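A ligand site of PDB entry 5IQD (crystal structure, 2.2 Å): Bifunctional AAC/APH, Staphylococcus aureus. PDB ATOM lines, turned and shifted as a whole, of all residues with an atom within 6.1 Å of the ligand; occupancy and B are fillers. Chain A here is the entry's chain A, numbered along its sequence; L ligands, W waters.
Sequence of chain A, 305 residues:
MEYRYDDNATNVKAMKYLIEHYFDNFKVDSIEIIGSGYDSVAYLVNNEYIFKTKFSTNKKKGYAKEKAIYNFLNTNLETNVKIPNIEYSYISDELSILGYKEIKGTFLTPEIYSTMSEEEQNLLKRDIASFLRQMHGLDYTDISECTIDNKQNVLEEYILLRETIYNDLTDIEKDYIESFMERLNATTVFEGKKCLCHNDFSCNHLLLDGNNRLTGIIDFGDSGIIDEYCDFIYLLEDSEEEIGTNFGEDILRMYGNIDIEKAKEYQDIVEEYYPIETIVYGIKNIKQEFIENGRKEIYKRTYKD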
ATOM      1  N   ASP A 200     -24.617  25.730  -4.443  1.00  0.00           N
ATOM      2  CA  ASP A 200     -24.469  24.731  -5.562  1.00  0.00           C
ATOM      3  C   ASP A 200     -25.877  24.314  -6.014  1.00  0.00           C
ATOM      4  O   ASP A 200     -26.220  23.130  -6.093  1.00  0.00           O
ATOM      5  CB  ASP A 200     -23.676  23.531  -5.087  1.00  0.00           C
ATOM      6  CG  ASP A 200     -23.074  22.748  -6.206  1.00  0.00           C
ATOM      7  OD1 ASP A 200     -23.106  23.204  -7.371  1.00  0.00           O
ATOM      8  OD2 ASP A 200     -22.510  21.692  -5.945  1.00  0.00           O
ATOM      9  N   PHE A 201     -26.685  25.303  -6.290  1.00  0.00           N
ATOM     10  CA  PHE A 201     -28.108  25.142  -6.328  1.00  0.00           C
ATOM     11  C   PHE A 201     -28.563  24.805  -7.746  1.00  0.00           C
ATOM     12  O   PHE A 201     -29.121  25.631  -8.445  1.00  0.00           O
ATOM     13  CB  PHE A 201     -28.789  26.384  -5.780  1.00  0.00           C
ATOM     14  CG  PHE A 201     -30.215  26.202  -5.355  1.00  0.00           C
ATOM     15  CD1 PHE A 201     -30.520  25.653  -4.146  1.00  0.00           C
ATOM     16  CD2 PHE A 201     -31.259  26.524  -6.197  1.00  0.00           C
ATOM     17  CE1 PHE A 201     -31.819  25.439  -3.748  1.00  0.00           C
ATOM     18  CE2 PHE A 201     -32.580  26.322  -5.797  1.00  0.00           C
ATOM     19  CZ  PHE A 201     -32.862  25.784  -4.572  1.00  0.00           C
ATOM     20  N   SER A 202     -28.366  23.544  -8.123  1.00  0.00           N
ATOM     21  CA  SER A 202     -28.655  23.060  -9.424  1.00  0.00           C
ATOM     22  C   SER A 202     -29.711  21.975  -9.337  1.00  0.00           C
ATOM     23  O   SER A 202     -29.961  21.472  -8.263  1.00  0.00           O
ATOM     24  CB  SER A 202     -27.405  22.498 -10.042  1.00  0.00           C
ATOM     25  OG  SER A 202     -26.769  21.612  -9.144  1.00  0.00           O
ATOM     26  N   ASN A 204     -29.874  18.836 -10.143  1.00  0.00           N
ATOM     27  CA  ASN A 204     -29.477  17.551  -9.599  1.00  0.00           C
ATOM     28  C   ASN A 204     -29.385  17.517  -8.027  1.00  0.00           C
ATOM     29  O   ASN A 204     -29.049  16.480  -7.461  1.00  0.00           O
ATOM     30  CB  ASN A 204     -28.183  17.086 -10.220  1.00  0.00           C
ATOM     31  CG  ASN A 204     -26.995  17.901  -9.740  1.00  0.00           C
ATOM     32  OD1 ASN A 204     -27.101  19.080  -9.513  1.00  0.00           O
ATOM     33  ND2 ASN A 204     -25.897  17.259  -9.512  1.00  0.00           N
ATOM     34  N   HIS A 205     -29.692  18.629  -7.356  1.00  0.00           N
ATOM     35  CA  HIS A 205     -29.780  18.657  -5.913  1.00  0.00           C
ATOM     36  C   HIS A 205     -31.180  18.942  -5.446  1.00  0.00           C
ATOM     37  O   HIS A 205     -31.387  19.095  -4.248  1.00  0.00           O
ATOM     38  CB  HIS A 205     -28.837  19.669  -5.294  1.00  0.00           C
ATOM     39  CG  HIS A 205     -27.409  19.351  -5.505  1.00  0.00           C
ATOM     40  ND1 HIS A 205     -26.453  20.314  -5.742  1.00  0.00           N
ATOM     41  CD2 HIS A 205     -26.762  18.168  -5.523  1.00  0.00           C
ATOM     42  CE1 HIS A 205     -25.264  19.729  -5.885  1.00  0.00           C
ATOM     43  NE2 HIS A 205     -25.432  18.421  -5.744  1.00  0.00           N
ATOM     44  N   ILE A 233     -27.313  30.989 -10.138  1.00  0.00           N
ATOM     45  CA  ILE A 233     -26.505  30.834 -11.314  1.00  0.00           C
ATOM     46  C   ILE A 233     -26.788  29.589 -12.096  1.00  0.00           C
ATOM     47  O   ILE A 233     -26.628  29.610 -13.335  1.00  0.00           O
ATOM     48  CB  ILE A 233     -25.002  30.982 -11.056  1.00  0.00           C
ATOM     49  CG1 ILE A 233     -24.487  29.837 -10.229  1.00  0.00           C
ATOM     50  CG2 ILE A 233     -24.714  32.309 -10.361  1.00  0.00           C
ATOM     51  CD1 ILE A 233     -23.003  29.826 -10.211  1.00  0.00           C
ATOM     52  N   TYR A 234     -27.259  28.549 -11.438  1.00  0.00           N
ATOM     53  CA  TYR A 234     -27.611  27.317 -12.223  1.00  0.00           C
ATOM     54  C   TYR A 234     -29.085  27.377 -12.661  1.00  0.00           C
ATOM     55  O   TYR A 234     -29.430  26.885 -13.738  1.00  0.00           O
ATOM     56  CB  TYR A 234     -27.239  26.050 -11.444  1.00  0.00           C
ATOM     57  CG  TYR A 234     -25.761  26.040 -11.089  1.00  0.00           C
ATOM     58  CD1 TYR A 234     -24.818  26.182 -12.048  1.00  0.00           C
ATOM     59  CD2 TYR A 234     -25.335  26.016  -9.766  1.00  0.00           C
ATOM     60  CE1 TYR A 234     -23.491  26.232 -11.746  1.00  0.00           C
ATOM     61  CE2 TYR A 234     -24.014  26.076  -9.443  1.00  0.00           C
ATOM     62  CZ  TYR A 234     -23.088  26.186 -10.430  1.00  0.00           C
ATOM     63  OH  TYR A 234     -21.747  26.255 -10.105  1.00  0.00           O
ATOM     64  N   GLU A 237     -29.005  28.899 -15.907  1.00  0.00           N
ATOM     65  CA  GLU A 237     -28.097  28.274 -16.900  1.00  0.00           C
ATOM     66  C   GLU A 237     -28.869  27.661 -18.049  1.00  0.00           C
ATOM     67  O   GLU A 237     -29.925  27.001 -17.873  1.00  0.00           O
ATOM     68  CB  GLU A 237     -27.222  27.225 -16.233  1.00  0.00           C
ATOM     69  CG  GLU A 237     -26.344  26.419 -17.125  1.00  0.00           C
ATOM     70  CD  GLU A 237     -25.430  25.518 -16.337  1.00  0.00           C
ATOM     71  OE1 GLU A 237     -24.588  26.077 -15.579  1.00  0.00           O
ATOM     72  OE2 GLU A 237     -25.501  24.274 -16.504  1.00  0.00           O
ATOM     73  N   ASP A 238     -28.347  27.871 -19.230  1.00  0.00           N
ATOM     74  CA  ASP A 238     -28.861  27.193 -20.441  1.00  0.00           C
ATOM     75  C   ASP A 238     -27.881  26.047 -20.785  1.00  0.00           C
ATOM     76  O   ASP A 238     -26.824  26.307 -21.305  1.00  0.00           O
ATOM     77  CB  ASP A 238     -28.970  28.230 -21.613  1.00  0.00           C
ATOM     78  CG  ASP A 238     -29.450  27.593 -22.925  1.00  0.00           C
ATOM     79  OD1 ASP A 238     -30.292  26.666 -22.884  1.00  0.00           O
ATOM     80  OD2 ASP A 238     -28.973  28.010 -23.999  1.00  0.00           O
ATOM     81  N   SER A 239     -28.257  24.813 -20.471  1.00  0.00           N
ATOM     82  CA  SER A 239     -27.442  23.618 -20.768  1.00  0.00           C
ATOM     83  C   SER A 239     -28.315  22.388 -20.766  1.00  0.00           C
ATOM     84  O   SER A 239     -29.458  22.433 -20.346  1.00  0.00           O
ATOM     85  CB  SER A 239     -26.393  23.451 -19.660  1.00  0.00           C
ATOM     86  OG  SER A 239     -27.014  23.160 -18.389  1.00  0.00           O
ATOM     87  N   GLU A 240     -27.749  21.261 -21.149  1.00  0.00           N
ATOM     88  CA  GLU A 240     -28.476  20.003 -21.091  1.00  0.00           C
ATOM     89  C   GLU A 240     -28.870  19.606 -19.671  1.00  0.00           C
ATOM     90  O   GLU A 240     -29.837  18.899 -19.474  1.00  0.00           O
ATOM     91  CB  GLU A 240     -27.674  18.866 -21.702  1.00  0.00           C
ATOM     92  CG  GLU A 240     -27.349  19.064 -23.163  1.00  0.00           C
ATOM     93  CD  GLU A 240     -27.052  17.765 -23.911  1.00  0.00           C
ATOM     94  OE1 GLU A 240     -26.760  17.880 -25.125  1.00  0.00           O
ATOM     95  OE2 GLU A 240     -27.122  16.658 -23.312  1.00  0.00           O
ATOM     96  N   GLU A 241     -28.061  19.979 -18.708  1.00  0.00           N
ATOM     97  CA  GLU A 241     -28.287  19.545 -17.315  1.00  0.00           C
ATOM     98  C   GLU A 241     -29.348  20.357 -16.563  1.00  0.00           C
ATOM     99  O   GLU A 241     -29.856  19.921 -15.545  1.00  0.00           O
ATOM    100  CB  GLU A 241     -26.979  19.672 -16.482  1.00  0.00           C
ATOM    101  CG  GLU A 241     -26.014  18.507 -16.558  1.00  0.00           C
ATOM    102  CD  GLU A 241     -24.656  18.789 -15.855  1.00  0.00           C
ATOM    103  OE1 GLU A 241     -24.508  19.784 -15.092  1.00  0.00           O
ATOM    104  OE2 GLU A 241     -23.726  17.972 -16.062  1.00  0.00           O
ATOM    105  N   GLU A 242     -29.594  21.575 -17.009  1.00  0.00           N
ATOM    106  CA  GLU A 242     -30.431  22.496 -16.283  1.00  0.00           C
ATOM    107  C   GLU A 242     -31.678  22.816 -17.114  1.00  0.00           C
ATOM    108  O   GLU A 242     -31.731  22.557 -18.295  1.00  0.00           O
ATOM    109  CB  GLU A 242     -29.683  23.764 -15.917  1.00  0.00           C
ATOM    110  CG  GLU A 242     -28.429  23.559 -15.083  1.00  0.00           C
ATOM    111  CD  GLU A 242     -28.616  22.842 -13.731  1.00  0.00           C
ATOM    112  OE1 GLU A 242     -29.646  23.015 -13.033  1.00  0.00           O
ATOM    113  OE2 GLU A 242     -27.689  22.080 -13.355  1.00  0.00           O
ATOM    114  N   GLN A 267     -23.800  35.202 -13.113  1.00  0.00           N
ATOM    115  CA  GLN A 267     -23.742  33.871 -13.736  1.00  0.00           C
ATOM    116  C   GLN A 267     -22.730  33.797 -14.907  1.00  0.00           C
ATOM    117  O   GLN A 267     -22.005  32.803 -15.067  1.00  0.00           O
ATOM    118  CB  GLN A 267     -25.119  33.529 -14.250  1.00  0.00           C
ATOM    119  CG  GLN A 267     -25.288  32.136 -14.782  1.00  0.00           C
ATOM    120  CD  GLN A 267     -25.005  32.052 -16.239  1.00  0.00           C
ATOM    121  OE1 GLN A 267     -25.265  32.988 -16.979  1.00  0.00           O
ATOM    122  NE2 GLN A 267     -24.473  30.881 -16.697  1.00  0.00           N
ATOM    123  N   VAL A 270     -19.115  33.721 -13.659  1.00  0.00           N
ATOM    124  CA  VAL A 270     -18.773  32.423 -13.102  1.00  0.00           C
ATOM    125  C   VAL A 270     -18.558  31.445 -14.201  1.00  0.00           C
ATOM    126  O   VAL A 270     -17.622  30.658 -14.188  1.00  0.00           O
ATOM    127  CB  VAL A 270     -19.848  31.934 -12.154  1.00  0.00           C
ATOM    128  CG1 VAL A 270     -19.673  30.444 -11.825  1.00  0.00           C
ATOM    129  CG2 VAL A 270     -19.793  32.762 -10.879  1.00  0.00           C
ATOM    130  N   GLU A 271     -19.407  31.522 -15.208  1.00  0.00           N
ATOM    131  CA  GLU A 271     -19.248  30.635 -16.370  1.00  0.00           C
ATOM    132  C   GLU A 271     -17.909  30.896 -17.112  1.00  0.00           C
ATOM    133  O   GLU A 271     -17.253  29.983 -17.520  1.00  0.00           O
ATOM    134  CB  GLU A 271     -20.428  30.764 -17.351  1.00  0.00           C
ATOM    135  CG  GLU A 271     -20.336  29.828 -18.607  1.00  0.00           C
ATOM    136  CD  GLU A 271     -20.506  28.325 -18.281  1.00  0.00           C
ATOM    137  OE1 GLU A 271     -19.523  27.549 -18.403  1.00  0.00           O
ATOM    138  OE2 GLU A 271     -21.610  27.918 -17.816  1.00  0.00           O
ATOM    139  N   GLU A 272     -17.546  32.144 -17.303  1.00  0.00           N
ATOM    140  CA  GLU A 272     -16.306  32.498 -17.968  1.00  0.00           C
ATOM    141  C   GLU A 272     -15.119  31.940 -17.181  1.00  0.00           C
ATOM    142  O   GLU A 272     -14.120  31.578 -17.732  1.00  0.00           O
ATOM    143  CB  GLU A 272     -16.224  34.022 -18.083  1.00  0.00           C
ATOM    144  CG  GLU A 272     -14.989  34.503 -18.915  1.00  0.00           C
ATOM    145  CD  GLU A 272     -14.971  35.996 -19.203  1.00  0.00           C
ATOM    146  OE1 GLU A 272     -16.054  36.610 -19.451  1.00  0.00           O
ATOM    147  OE2 GLU A 272     -13.874  36.565 -19.373  1.00  0.00           O
ATOM    148  N   TYR A 274     -14.969  29.184 -15.447  1.00  0.00           N
ATOM    149  CA  TYR A 274     -14.952  27.734 -15.378  1.00  0.00           C
ATOM    150  C   TYR A 274     -13.662  27.071 -15.827  1.00  0.00           C
ATOM    151  O   TYR A 274     -13.153  26.212 -15.127  1.00  0.00           O
ATOM    152  CB  TYR A 274     -16.148  27.156 -16.158  1.00  0.00           C
ATOM    153  CG  TYR A 274     -16.385  25.649 -16.059  1.00  0.00           C
ATOM    154  CD1 TYR A 274     -15.935  24.879 -14.990  1.00  0.00           C
ATOM    155  CD2 TYR A 274     -17.189  25.015 -17.009  1.00  0.00           C
ATOM    156  CE1 TYR A 274     -16.197  23.511 -14.939  1.00  0.00           C
ATOM    157  CE2 TYR A 274     -17.476  23.669 -16.956  1.00  0.00           C
ATOM    158  CZ  TYR A 274     -16.990  22.924 -15.920  1.00  0.00           C
ATOM    159  OH  TYR A 274     -17.339  21.580 -15.892  1.00  0.00           O
ATOM    160  N   GLU A 277     -11.031  27.795 -13.292  1.00  0.00           N
ATOM    161  CA  GLU A 277     -11.344  26.979 -12.067  1.00  0.00           C
ATOM    162  C   GLU A 277     -10.824  25.530 -12.220  1.00  0.00           C
ATOM    163  O   GLU A 277     -10.226  24.970 -11.295  1.00  0.00           O
ATOM    164  CB  GLU A 277     -12.833  26.941 -11.828  1.00  0.00           C
ATOM    165  CG  GLU A 277     -13.297  25.983 -10.717  1.00  0.00           C
ATOM    166  CD  GLU A 277     -14.803  25.788 -10.705  1.00  0.00           C
ATOM    167  OE1 GLU A 277     -15.328  24.792 -11.277  1.00  0.00           O
ATOM    168  OE2 GLU A 277     -15.447  26.674 -10.142  1.00  0.00           O
ATOM    169  N   ARG A 301     -13.704  27.768 -26.306  1.00  0.00           N
ATOM    170  CA  ARG A 301     -14.465  29.002 -26.099  1.00  0.00           C
ATOM    171  C   ARG A 301     -13.958  30.140 -27.000  1.00  0.00           C
ATOM    172  O   ARG A 301     -14.731  30.927 -27.527  1.00  0.00           O
ATOM    173  CB  ARG A 301     -14.446  29.388 -24.634  1.00  0.00           C
ATOM    174  CG  ARG A 301     -15.411  28.601 -23.782  1.00  0.00           C
ATOM    175  CD  ARG A 301     -14.929  28.621 -22.361  1.00  0.00           C
ATOM    176  NE  ARG A 301     -15.903  28.891 -21.296  1.00  0.00           N
ATOM    177  CZ  ARG A 301     -16.556  27.989 -20.625  1.00  0.00           C
ATOM    178  NH1 ARG A 301     -16.425  26.708 -20.891  1.00  0.00           N
ATOM    179  NH2 ARG A 301     -17.345  28.377 -19.688  1.00  0.00           N
HETATM  180  O1  LIG L   1     -20.883  28.008 -14.645  1.00  0.00           O
HETATM  181  C1  LIG L   1     -19.600  27.527 -14.268  1.00  0.00           C
HETATM  182  C2  LIG L   1     -19.674  26.689 -13.013  1.00  0.00           C
HETATM  183  O2  LIG L   1     -20.497  25.548 -13.305  1.00  0.00           O
HETATM  184  C3  LIG L   1     -20.051  24.570 -12.347  1.00  0.00           C
HETATM  185  O3  LIG L   1     -20.478  23.243 -12.642  1.00  0.00           O
HETATM  186  C4  LIG L   1     -21.876  23.052 -12.367  1.00  0.00           C
HETATM  187  C5  LIG L   1     -22.091  22.262 -11.092  1.00  0.00           C
HETATM  188  O4  LIG L   1     -21.333  22.864 -10.011  1.00  0.00           O
HETATM  189  C6  LIG L   1     -23.609  22.294 -10.786  1.00  0.00           C
HETATM  190  N1  LIG L   1     -23.973  21.646  -9.513  1.00  0.00           N
HETATM  191  C7  LIG L   1     -24.381  21.733 -11.973  1.00  0.00           C
HETATM  192  C8  LIG L   1     -24.127  22.575 -13.228  1.00  0.00           C
HETATM  193  N2  LIG L   1     -25.011  22.178 -14.332  1.00  0.00           N
HETATM  194  C9  LIG L   1     -22.633  22.518 -13.576  1.00  0.00           C
HETATM  195  O5  LIG L   1     -22.508  23.386 -14.737  1.00  0.00           O
HETATM  196  C10 LIG L   1     -21.284  23.441 -15.467  1.00  0.00           C
HETATM  197  O6  LIG L   1     -20.884  22.177 -15.948  1.00  0.00           O
HETATM  198  C11 LIG L   1     -21.717  21.611 -16.984  1.00  0.00           C
HETATM  199  C12 LIG L   1     -21.101  20.275 -17.365  1.00  0.00           C
HETATM  200  N3  LIG L   1     -21.493  19.344 -16.324  1.00  0.00           N
HETATM  201  C13 LIG L   1     -21.826  22.535 -18.189  1.00  0.00           C
HETATM  202  O7  LIG L   1     -22.759  21.964 -19.131  1.00  0.00           O
HETATM  203  C14 LIG L   1     -22.285  23.903 -17.734  1.00  0.00           C
HETATM  204  O8  LIG L   1     -22.352  24.777 -18.830  1.00  0.00           O
HETATM  205  C15 LIG L   1     -21.383  24.451 -16.615  1.00  0.00           C
HETATM  206  N4  LIG L   1     -21.927  25.707 -16.125  1.00  0.00           N
HETATM  207  C16 LIG L   1     -18.535  24.627 -12.485  1.00  0.00           C
HETATM  208  O9  LIG L   1     -17.859  23.991 -11.423  1.00  0.00           O
HETATM  209  C17 LIG L   1     -18.318  26.152 -12.509  1.00  0.00           C
HETATM  210  O10 LIG L   1     -17.942  26.653 -11.213  1.00  0.00           O
HETATM  211  O   HOH W   1     -24.915  20.106 -18.774  1.00  0.00           O
HETATM  212  O   HOH W   2     -22.404  29.851 -14.076  1.00  0.00           O
HETATM  213  O   HOH W   3     -20.918  21.002  -7.922  1.00  0.00           O
HETATM  214  O   HOH W   4     -23.062  18.810  -9.542  1.00  0.00           O
HETATM  215  O   HOH W   5     -23.555  22.958 -21.673  1.00  0.00           O
HETATM  216  O   HOH W   6     -18.628  24.446  -8.458  1.00  0.00           O
HETATM  217  O   HOH W   7     -21.056  25.047  -8.003  1.00  0.00           O
HETATM  218  O   HOH W   8     -24.030  26.450 -20.108  1.00  0.00           O
HETATM  219  O   HOH W   9     -19.924  25.100 -19.430  1.00  0.00           O
HETATM  220  O   HOH W  10     -16.539  28.801 -12.529  1.00  0.00           O
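The side-chain carboxylate (OD1) of Asp 200 is in salt-bridge range of a nitrogen (N1) of the ligand (2.8 Å). The side-chain carboxylate of Glu 237 is in salt-bridge range of a nitrogen (N4) of the ligand (2.7 Å). A nitrogen (N2) of the ligand lies within salt-bridge range of the side-chain carboxylate (OE1) of Glu 241. OH of Tyr 234 sits close to O4 of the ligand, 3.4 Å away. An oxygen (O9) of the ligand is in hydrogen-bond range of the side-chain carboxylate of Glu 277, 2.7 Å away. OG of Ser 202 sits at hydrogen-bond distance from N1 of the ligand (2.8 Å). The side-chain carboxylate (OE2) of Glu 271 is in salt-bridge range of a nitrogen (N4) of the ligand (2.8 Å). N2 of the ligand lies within salt-bridge range of OE2 of Glu 242, at 2.9 Å.
The backbone NH of Glu 242 sits at hydrogen-bond distance from the side-chain hydroxyl of Ser 239, at 3.3 Å. The backbone carbonyl oxygen (O) of Asp 200 lies within hydrogen-bond range of the side-chain hydroxyl (OG) of Ser 202, 3.5 Å away. OE2 of Glu 237 sits at hydrogen-bond distance from OG of Ser 239 (2.7 Å). The side-chain hydroxyl of Ser 239 sits close to the backbone NH of Glu 241 (3.4 Å). O of Asp 200 sits at hydrogen-bond distance from ND1 of His 205 (2.8 Å). NH2 of Arg 301 lies within salt-bridge range of OE1 of Glu 271. OG of Ser 202 lies within hydrogen-bond range of OD1 of Asn 204 (2.6 Å).
Ser 239 touches the ligand (CB to O7, 3.96 Å). O of Val 270 touches C1 of the ligand, at 3.7 Å. Tyr 274 touches the ligand (CE1 to C16, 3.6 Å). Hydrophobic or aromatic side chains that line the ligand: Tyr 234, Val 270 and Tyr 274.
Water W2 bridges an oxygen (O1) of the ligand and the backbone carbonyl oxygen (O) of Gln 267. Water W9 bridges O8 of the ligand (2.5 Å) and OE1 of Glu 271 (2.7 Å). Water W8 lies within hydrogen-bond range of an oxygen (O8) of the ligand (2.7 Å) and the backbone carbonyl oxygen (O) of Asp 238 (3.0 Å). Water W3 lies within hydrogen-bond range of OD2 of Asp 200 (2.6 Å) and O4 of the ligand (2.8 Å). Water W4 bridges a nitrogen (N1) of the ligand (3.0 Å) and the side-chain amide nitrogen (ND2) of Asn 204 (3.2 Å). Water W7 lies within hydrogen-bond range of the side-chain hydroxyl (OH) of Tyr 234 (2.5 Å), the side-chain carboxylate (OD1) of Asp 200 (2.8 Å) and an oxygen (O4) of the ligand (3.0 Å).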
